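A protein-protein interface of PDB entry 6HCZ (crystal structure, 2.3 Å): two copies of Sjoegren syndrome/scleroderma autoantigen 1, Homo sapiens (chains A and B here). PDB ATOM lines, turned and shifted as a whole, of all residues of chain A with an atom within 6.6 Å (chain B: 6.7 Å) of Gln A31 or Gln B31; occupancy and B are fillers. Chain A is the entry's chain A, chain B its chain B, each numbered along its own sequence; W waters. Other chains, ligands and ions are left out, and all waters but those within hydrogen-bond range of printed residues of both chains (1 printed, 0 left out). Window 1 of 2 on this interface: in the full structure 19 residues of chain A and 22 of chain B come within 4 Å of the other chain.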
ATOM      1  N   ALA A  26       4.898  33.552  20.163  1.00  0.00           N
ATOM      2  CA  ALA A  26       5.899  32.890  20.983  1.00  0.00           C
ATOM      3  C   ALA A  26       5.480  31.454  21.322  1.00  0.00           C
ATOM      4  O   ALA A  26       6.296  30.545  21.133  1.00  0.00           O
ATOM      5  CB  ALA A  26       6.126  33.665  22.251  1.00  0.00           C
ATOM      6  N   ARG A  27       4.239  31.267  21.818  1.00  0.00           N
ATOM      7  CA  ARG A  27       3.786  29.953  22.328  1.00  0.00           C
ATOM      8  C   ARG A  27       3.702  28.987  21.148  1.00  0.00           C
ATOM      9  O   ARG A  27       3.998  27.797  21.243  1.00  0.00           O
ATOM     10  CB  ARG A  27       2.439  30.037  23.068  1.00  0.00           C
ATOM     11  CG  ARG A  27       1.244  29.568  22.246  1.00  0.00           C
ATOM     12  CD  ARG A  27       0.160  28.860  23.014  1.00  0.00           C
ATOM     13  NE  ARG A  27       0.575  27.600  23.604  1.00  0.00           N
ATOM     14  CZ  ARG A  27       0.226  26.407  23.146  1.00  0.00           C
ATOM     15  NH1 ARG A  27      -0.117  26.236  21.886  1.00  0.00           N
ATOM     16  NH2 ARG A  27       0.203  25.377  23.957  1.00  0.00           N
ATOM     17  N   ARG A  28       3.248  29.535  20.030  1.00  0.00           N
ATOM     18  CA  ARG A  28       3.130  28.851  18.822  1.00  0.00           C
ATOM     19  C   ARG A  28       4.520  28.426  18.330  1.00  0.00           C
ATOM     20  O   ARG A  28       4.711  27.300  17.941  1.00  0.00           O
ATOM     21  CB  ARG A  28       2.367  29.816  17.924  1.00  0.00           C
ATOM     22  CG  ARG A  28       2.046  29.335  16.524  1.00  0.00           C
ATOM     23  CD  ARG A  28       1.193  30.433  15.912  1.00  0.00           C
ATOM     24  NE  ARG A  28      -0.058  29.890  15.436  1.00  0.00           N
ATOM     25  CZ  ARG A  28      -1.256  30.400  15.672  1.00  0.00           C
ATOM     26  NH1 ARG A  28      -1.391  31.628  16.179  1.00  0.00           N
ATOM     27  NH2 ARG A  28      -2.307  29.652  15.359  1.00  0.00           N
ATOM     28  N   GLU A  29       5.502  29.327  18.373  1.00  0.00           N
ATOM     29  CA  GLU A  29       6.886  28.981  17.973  1.00  0.00           C
ATOM     30  C   GLU A  29       7.450  27.908  18.920  1.00  0.00           C
ATOM     31  O   GLU A  29       7.990  26.924  18.459  1.00  0.00           O
ATOM     32  CB  GLU A  29       7.789  30.225  17.918  1.00  0.00           C
ATOM     33  CG  GLU A  29       8.043  30.755  16.510  1.00  0.00           C
ATOM     34  CD  GLU A  29       7.874  32.265  16.303  1.00  0.00           C
ATOM     35  OE1 GLU A  29       7.855  32.708  15.125  1.00  0.00           O
ATOM     36  OE2 GLU A  29       7.746  33.012  17.304  1.00  0.00           O
ATOM     37  N   ARG A  30       7.314  28.109  20.233  1.00  0.00           N
ATOM     38  CA  ARG A  30       7.765  27.142  21.222  1.00  0.00           C
ATOM     39  C   ARG A  30       7.264  25.750  20.835  1.00  0.00           C
ATOM     40  O   ARG A  30       8.021  24.794  20.720  1.00  0.00           O
ATOM     41  CB  ARG A  30       7.259  27.521  22.609  1.00  0.00           C
ATOM     42  CG  ARG A  30       8.030  26.921  23.772  1.00  0.00           C
ATOM     43  CD  ARG A  30       7.210  26.824  25.054  1.00  0.00           C
ATOM     44  NE  ARG A  30       8.055  26.389  26.153  1.00  0.00           N
ATOM     45  CZ  ARG A  30       7.860  25.336  26.952  1.00  0.00           C
ATOM     46  NH1 ARG A  30       6.653  24.805  27.078  1.00  0.00           N
ATOM     47  NH2 ARG A  30       8.890  24.853  27.648  1.00  0.00           N
ATOM     48  N   GLN A  31       5.964  25.648  20.604  1.00  0.00           N
ATOM     49  CA  GLN A  31       5.375  24.390  20.409  1.00  0.00           C
ATOM     50  C   GLN A  31       5.901  23.771  19.129  1.00  0.00           C
ATOM     51  O   GLN A  31       6.099  22.567  19.099  1.00  0.00           O
ATOM     52  CB  GLN A  31       3.851  24.495  20.421  1.00  0.00           C
ATOM     53  CG  GLN A  31       3.315  24.560  21.838  1.00  0.00           C
ATOM     54  CD  GLN A  31       3.755  23.377  22.674  1.00  0.00           C
ATOM     55  OE1 GLN A  31       4.063  22.295  22.170  1.00  0.00           O
ATOM     56  NE2 GLN A  31       3.808  23.575  23.974  1.00  0.00           N
ATOM     57  N   ASP A  32       6.140  24.582  18.099  1.00  0.00           N
ATOM     58  CA  ASP A  32       6.623  24.050  16.844  1.00  0.00           C
ATOM     59  C   ASP A  32       8.027  23.484  17.025  1.00  0.00           C
ATOM     60  O   ASP A  32       8.349  22.427  16.478  1.00  0.00           O
ATOM     61  CB  ASP A  32       6.629  25.055  15.695  1.00  0.00           C
ATOM     62  CG  ASP A  32       7.147  24.410  14.404  1.00  0.00           C
ATOM     63  OD1 ASP A  32       6.719  23.249  14.101  1.00  0.00           O
ATOM     64  OD2 ASP A  32       8.015  25.027  13.727  1.00  0.00           O
ATOM     65  N   ARG A  33       8.844  24.196  17.798  1.00  0.00           N
ATOM     66  CA  ARG A  33      10.198  23.789  18.108  1.00  0.00           C
ATOM     67  C   ARG A  33      10.177  22.533  18.976  1.00  0.00           C
ATOM     68  O   ARG A  33      10.939  21.626  18.733  1.00  0.00           O
ATOM     69  CB  ARG A  33      10.957  24.953  18.751  1.00  0.00           C
ATOM     70  CG  ARG A  33      11.475  25.949  17.723  1.00  0.00           C
ATOM     71  CD  ARG A  33      12.462  26.923  18.322  1.00  0.00           C
ATOM     72  NE  ARG A  33      11.804  28.117  18.845  1.00  0.00           N
ATOM     73  CZ  ARG A  33      11.922  29.344  18.330  1.00  0.00           C
ATOM     74  NH1 ARG A  33      12.720  29.550  17.293  1.00  0.00           N
ATOM     75  NH2 ARG A  33      11.242  30.353  18.860  1.00  0.00           N
ATOM     76  N   ILE A  34       9.300  22.468  19.973  1.00  0.00           N
ATOM     77  CA  ILE A  34       9.200  21.245  20.785  1.00  0.00           C
ATOM     78  C   ILE A  34       8.961  20.052  19.849  1.00  0.00           C
ATOM     79  O   ILE A  34       9.622  18.991  19.969  1.00  0.00           O
ATOM     80  CB  ILE A  34       8.110  21.364  21.877  1.00  0.00           C
ATOM     81  CG1 ILE A  34       8.507  22.341  22.978  1.00  0.00           C
ATOM     82  CG2 ILE A  34       7.743  20.013  22.490  1.00  0.00           C
ATOM     83  CD1 ILE A  34       7.316  22.848  23.786  1.00  0.00           C
ATOM     84  N   SER A  35       8.047  20.207  18.893  1.00  0.00           N
ATOM     85  CA  SER A  35       7.712  19.053  18.039  1.00  0.00           C
ATOM     86  C   SER A  35       8.907  18.656  17.168  1.00  0.00           C
ATOM     87  O   SER A  35       9.190  17.480  17.010  1.00  0.00           O
ATOM     88  CB  SER A  35       6.493  19.305  17.188  1.00  0.00           C
ATOM     89  OG  SER A  35       5.352  19.451  18.010  1.00  0.00           O
ATOM     90  N   ARG A  36       9.583  19.661  16.605  1.00  0.00           N
ATOM     91  CA  ARG A  36      10.719  19.470  15.741  1.00  0.00           C
ATOM     92  C   ARG A  36      11.839  18.771  16.528  1.00  0.00           C
ATOM     93  O   ARG A  36      12.397  17.739  16.089  1.00  0.00           O
ATOM     94  CB  ARG A  36      11.117  20.818  15.119  1.00  0.00           C
ATOM     95  CG  ARG A  36      12.405  20.759  14.294  1.00  0.00           C
ATOM     96  CD  ARG A  36      12.627  21.890  13.289  1.00  0.00           C
ATOM     97  NE  ARG A  36      12.082  23.168  13.731  1.00  0.00           N
ATOM     98  CZ  ARG A  36      10.850  23.596  13.465  1.00  0.00           C
ATOM     99  NH1 ARG A  36      10.067  22.915  12.642  1.00  0.00           N
ATOM    100  NH2 ARG A  36      10.405  24.709  14.026  1.00  0.00           N
ATOM    101  N   CYS A  56       5.883  20.904  32.727  1.00  0.00           N
ATOM    102  CA  CYS A  56       5.488  21.642  31.489  1.00  0.00           C
ATOM    103  C   CYS A  56       4.487  20.897  30.575  1.00  0.00           C
ATOM    104  O   CYS A  56       3.993  21.498  29.661  1.00  0.00           O
ATOM    105  CB  CYS A  56       6.730  22.015  30.682  1.00  0.00           C
ATOM    106  SG  CYS A  56       7.357  20.673  29.642  1.00  0.00           S
ATOM    107  N   THR A  58       4.878  18.447  28.334  1.00  0.00           N
ATOM    108  CA  THR A  58       5.456  17.821  27.141  1.00  0.00           C
ATOM    109  C   THR A  58       5.697  16.311  27.332  1.00  0.00           C
ATOM    110  O   THR A  58       6.200  15.880  28.372  1.00  0.00           O
ATOM    111  CB  THR A  58       6.808  18.473  26.829  1.00  0.00           C
ATOM    112  OG1 THR A  58       6.576  19.871  26.776  1.00  0.00           O
ATOM    113  CG2 THR A  58       7.431  17.996  25.538  1.00  0.00           C
ATOM    114  N   ALA B  26       0.062  13.572  16.348  1.00  0.00           N
ATOM    115  CA  ALA B  26      -1.135  13.953  17.135  1.00  0.00           C
ATOM    116  C   ALA B  26      -0.835  15.188  17.989  1.00  0.00           C
ATOM    117  O   ALA B  26      -1.564  16.144  18.064  1.00  0.00           O
ATOM    118  CB  ALA B  26      -1.527  12.817  18.019  1.00  0.00           C
ATOM    119  N   ARG B  27       0.304  15.104  18.650  1.00  0.00           N
ATOM    120  CA  ARG B  27       0.777  16.082  19.565  1.00  0.00           C
ATOM    121  C   ARG B  27       0.965  17.400  18.832  1.00  0.00           C
ATOM    122  O   ARG B  27       0.674  18.443  19.347  1.00  0.00           O
ATOM    123  CB  ARG B  27       2.082  15.533  20.128  1.00  0.00           C
ATOM    124  CG  ARG B  27       2.784  16.460  21.090  1.00  0.00           C
ATOM    125  CD  ARG B  27       3.988  17.143  20.511  1.00  0.00           C
ATOM    126  NE  ARG B  27       4.363  17.909  21.675  1.00  0.00           N
ATOM    127  CZ  ARG B  27       4.381  19.224  21.773  1.00  0.00           C
ATOM    128  NH1 ARG B  27       4.242  19.765  22.963  1.00  0.00           N
ATOM    129  NH2 ARG B  27       4.632  19.988  20.727  1.00  0.00           N
ATOM    130  N   ARG B  28       1.443  17.289  17.594  1.00  0.00           N
ATOM    131  CA  ARG B  28       1.641  18.402  16.680  1.00  0.00           C
ATOM    132  C   ARG B  28       0.278  19.027  16.386  1.00  0.00           C
ATOM    133  O   ARG B  28       0.124  20.196  16.540  1.00  0.00           O
ATOM    134  CB  ARG B  28       2.317  17.903  15.392  1.00  0.00           C
ATOM    135  CG  ARG B  28       3.094  18.941  14.596  1.00  0.00           C
ATOM    136  CD  ARG B  28       3.892  18.271  13.479  1.00  0.00           C
ATOM    137  NE  ARG B  28       5.346  18.223  13.651  1.00  0.00           N
ATOM    138  CZ  ARG B  28       6.067  17.101  13.548  1.00  0.00           C
ATOM    139  NH1 ARG B  28       5.469  15.903  13.474  1.00  0.00           N
ATOM    140  NH2 ARG B  28       7.391  17.189  13.464  1.00  0.00           N
ATOM    141  N   GLU B  29      -0.694  18.215  15.954  1.00  0.00           N
ATOM    142  CA  GLU B  29      -1.991  18.722  15.522  1.00  0.00           C
ATOM    143  C   GLU B  29      -2.680  19.400  16.694  1.00  0.00           C
ATOM    144  O   GLU B  29      -3.171  20.491  16.554  1.00  0.00           O
ATOM    145  CB  GLU B  29      -2.845  17.595  14.951  1.00  0.00           C
ATOM    146  CG  GLU B  29      -2.327  17.106  13.607  1.00  0.00           C
ATOM    147  CD  GLU B  29      -3.213  16.125  12.867  1.00  0.00           C
ATOM    148  OE1 GLU B  29      -3.969  15.386  13.534  1.00  0.00           O
ATOM    149  OE2 GLU B  29      -3.139  16.106  11.621  1.00  0.00           O
ATOM    150  N   ARG B  30      -2.613  18.764  17.866  1.00  0.00           N
ATOM    151  CA  ARG B  30      -3.185  19.284  19.067  1.00  0.00           C
ATOM    152  C   ARG B  30      -2.657  20.687  19.390  1.00  0.00           C
ATOM    153  O   ARG B  30      -3.388  21.567  19.792  1.00  0.00           O
ATOM    154  CB  ARG B  30      -2.840  18.362  20.240  1.00  0.00           C
ATOM    155  CG  ARG B  30      -3.541  18.770  21.521  1.00  0.00           C
ATOM    156  CD  ARG B  30      -3.586  17.731  22.612  1.00  0.00           C
ATOM    157  NE  ARG B  30      -2.736  18.176  23.703  1.00  0.00           N
ATOM    158  CZ  ARG B  30      -3.137  18.707  24.843  1.00  0.00           C
ATOM    159  NH1 ARG B  30      -4.428  18.766  25.148  1.00  0.00           N
ATOM    160  NH2 ARG B  30      -2.214  19.141  25.684  1.00  0.00           N
ATOM    161  N   GLN B  31      -1.336  20.850  19.352  1.00  0.00           N
ATOM    162  CA  GLN B  31      -0.768  22.090  19.747  1.00  0.00           C
ATOM    163  C   GLN B  31      -1.187  23.140  18.725  1.00  0.00           C
ATOM    164  O   GLN B  31      -1.527  24.252  19.091  1.00  0.00           O
ATOM    165  CB  GLN B  31       0.748  21.984  19.904  1.00  0.00           C
ATOM    166  CG  GLN B  31       1.193  21.467  21.269  1.00  0.00           C
ATOM    167  CD  GLN B  31       0.757  22.359  22.405  1.00  0.00           C
ATOM    168  OE1 GLN B  31       0.411  23.513  22.207  1.00  0.00           O
ATOM    169  NE2 GLN B  31       0.798  21.843  23.617  1.00  0.00           N
ATOM    170  N   ASP B  32      -1.235  22.757  17.448  1.00  0.00           N
ATOM    171  CA  ASP B  32      -1.682  23.667  16.399  1.00  0.00           C
ATOM    172  C   ASP B  32      -3.105  24.154  16.732  1.00  0.00           C
ATOM    173  O   ASP B  32      -3.398  25.342  16.651  1.00  0.00           O
ATOM    174  CB  ASP B  32      -1.491  23.023  15.020  1.00  0.00           C
ATOM    175  CG  ASP B  32      -0.020  22.728  14.684  1.00  0.00           C
ATOM    176  OD1 ASP B  32       0.878  23.103  15.497  1.00  0.00           O
ATOM    177  OD2 ASP B  32       0.242  22.117  13.608  1.00  0.00           O
ATOM    178  N   ARG B  33      -3.969  23.235  17.170  1.00  0.00           N
ATOM    179  CA  ARG B  33      -5.366  23.530  17.462  1.00  0.00           C
ATOM    180  C   ARG B  33      -5.457  24.452  18.688  1.00  0.00           C
ATOM    181  O   ARG B  33      -6.266  25.380  18.749  1.00  0.00           O
ATOM    182  CB  ARG B  33      -6.113  22.203  17.653  1.00  0.00           C
ATOM    183  CG  ARG B  33      -7.365  22.054  16.797  1.00  0.00           C
ATOM    184  CD  ARG B  33      -7.484  20.674  16.173  1.00  0.00           C
ATOM    185  NE  ARG B  33      -7.193  19.602  17.121  1.00  0.00           N
ATOM    186  CZ  ARG B  33      -6.848  18.348  16.799  1.00  0.00           C
ATOM    187  NH1 ARG B  33      -6.816  17.949  15.532  1.00  0.00           N
ATOM    188  NH2 ARG B  33      -6.523  17.501  17.761  1.00  0.00           N
ATOM    189  N   ILE B  34      -4.600  24.214  19.678  1.00  0.00           N
ATOM    190  CA  ILE B  34      -4.643  24.991  20.894  1.00  0.00           C
ATOM    191  C   ILE B  34      -4.265  26.439  20.583  1.00  0.00           C
ATOM    192  O   ILE B  34      -4.934  27.345  21.035  1.00  0.00           O
ATOM    193  CB  ILE B  34      -3.730  24.384  21.976  1.00  0.00           C
ATOM    194  CG1 ILE B  34      -4.354  23.162  22.641  1.00  0.00           C
ATOM    195  CG2 ILE B  34      -3.349  25.407  23.025  1.00  0.00           C
ATOM    196  CD1 ILE B  34      -3.321  22.295  23.330  1.00  0.00           C
ATOM    197  N   SER B  35      -3.188  26.643  19.820  1.00  0.00           N
ATOM    198  CA  SER B  35      -2.795  27.992  19.363  1.00  0.00           C
ATOM    199  C   SER B  35      -3.942  28.659  18.586  1.00  0.00           C
ATOM    200  O   SER B  35      -4.177  29.839  18.744  1.00  0.00           O
ATOM    201  CB  SER B  35      -1.545  27.954  18.531  1.00  0.00           C
ATOM    202  OG  SER B  35      -0.409  27.614  19.310  1.00  0.00           O
ATOM    203  N   ARG B  36      -4.650  27.898  17.748  1.00  0.00           N
ATOM    204  CA  ARG B  36      -5.681  28.452  16.907  1.00  0.00           C
ATOM    205  C   ARG B  36      -6.878  28.856  17.781  1.00  0.00           C
ATOM    206  O   ARG B  36      -7.388  29.943  17.650  1.00  0.00           O
ATOM    207  CB  ARG B  36      -5.976  27.469  15.765  1.00  0.00           C
ATOM    208  CG  ARG B  36      -7.008  27.958  14.750  1.00  0.00           C
ATOM    209  CD  ARG B  36      -6.872  27.304  13.379  1.00  0.00           C
ATOM    210  NE  ARG B  36      -7.020  25.850  13.391  1.00  0.00           N
ATOM    211  CZ  ARG B  36      -6.017  24.978  13.414  1.00  0.00           C
ATOM    212  NH1 ARG B  36      -4.765  25.378  13.243  1.00  0.00           N
ATOM    213  NH2 ARG B  36      -6.273  23.700  13.636  1.00  0.00           N
ATOM    214  N   CYS B  56      -2.167  21.047  32.260  1.00  0.00           N
ATOM    215  CA  CYS B  56      -1.657  20.733  30.920  1.00  0.00           C
ATOM    216  C   CYS B  56      -0.589  21.716  30.429  1.00  0.00           C
ATOM    217  O   CYS B  56       0.027  21.483  29.397  1.00  0.00           O
ATOM    218  CB  CYS B  56      -2.787  20.794  29.913  1.00  0.00           C
ATOM    219  SG  CYS B  56      -3.184  22.510  29.517  1.00  0.00           S
ATOM    220  N   THR B  58      -1.008  24.887  29.437  1.00  0.00           N
ATOM    221  CA  THR B  58      -1.511  25.873  28.474  1.00  0.00           C
ATOM    222  C   THR B  58      -1.756  27.226  29.155  1.00  0.00           C
ATOM    223  O   THR B  58      -2.363  27.275  30.204  1.00  0.00           O
ATOM    224  CB  THR B  58      -2.820  25.392  27.843  1.00  0.00           C
ATOM    225  OG1 THR B  58      -2.489  24.180  27.175  1.00  0.00           O
ATOM    226  CG2 THR B  58      -3.419  26.390  26.880  1.00  0.00           C
HETATM  227  O   HOH W   1      -0.102  23.310  26.372  1.00  0.00           O
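Hydrophobic or aromatic side chains of chain A that line the printed part of chain B: Ile A34.
Of the 13 printed residues of chain B, 7 touch a printed residue of chain A.
Hydrophobic or aromatic side chains of chain B that line the printed part of chain A: Ile B34.
Along chain B the printed residues that touch a printed residue of chain A span positions 27 to 56.
Among the printed residues, 11 pairs touch across the chains.
Arg A27 touches Ile B34, and with the chains exchanged Ile A34 touches Arg B27.
Arg A27 touches Ser B35, and with the chains exchanged Ser A35 touches Arg B27.
Arg A28 touches Arg B36, but with the chains exchanged Arg A36 does not touch Arg B28 (4.6 Å).
Cys B56 touches its own counterpart, Cys A56.
Of the 11 pairs that touch across the chains among the printed residues, 10 have their exchanged pair printed and touching as well.
NH2 of Arg A27 sits at hydrogen-bond distance from OE1 of Gln B31, at 2.6 Å.
The guanidinium group (NH1) of Arg A27 lies within hydrogen-bond range of the side-chain hydroxyl (OG) of Ser B35.
The guanidinium group (NH1) of Arg B27 is in hydrogen-bond range of the side-chain amide oxygen (OE1) of Gln A31 (2.7 Å).
The side-chain amide nitrogen (NE2) of Gln A31 lies close to the side-chain amide nitrogen (NE2) of Gln B31, at 3.5 Å.
The guanidinium group (NH2) of Arg B27 is in hydrogen-bond range of the side-chain hydroxyl (OG) of Ser A35 (2.9 Å).
Among the printed residues, pairs that only touch across the chains: Arg A27 with Ile B34, Ile A34 with Arg B27, Arg A28 with Ser B35, Arg A28 with Arg B36, Ser A35 with Arg B28 and Cys A56 with Cys B56.
Of the printed residues of chain B, Arg A28 touches Ser B35 (3.7 Å) and Arg B36 (3.8 Å).
Gln A31 touches just these residues of chain B: Arg B27 (2.7 Å) and Gln B31 (3.1 Å).
Of the printed residues of chain B, Ile A34 touches Arg B27.
Of the printed residues of chain B, Cys A56 touches Cys B56.
Gln B31 touches just these residues of chain A: Arg A27 (2.6 Å) and Gln A31 (3.1 Å).
Of the printed residues of chain A, Ser B35 touches Arg A27 (2.9 Å) and Arg A28 (3.7 Å).
Of the printed residues of chain A, Cys B56 touches Cys A56.
The nearest residue of chain B that does not touch Gln A31 is Ser B35 (5.4 Å).
The nearest residue of chain A that does not touch Gln B31 is Ser A35 (5.6 Å).
The nearest printed residue of chain A that does not touch Arg B36 is Arg A27 (6.4 Å).
Water W1 lies within hydrogen-bond range of the side-chain hydroxyl of Thr B58 (2.7 Å), the guanidinium group of Arg A27 (3.2 Å) and the side-chain amide nitrogen of Gln B31 (3.2 Å).
O of Gln A31 is in hydrogen-bond range of OG of Ser A35.
SG of Cys A56 lies close to OG1 of Thr A58 (3.1 Å).
The side-chain sulfur (SG) of Cys B56 sits close to the side-chain hydroxyl (OG1) of Thr B58, at 3.0 Å.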
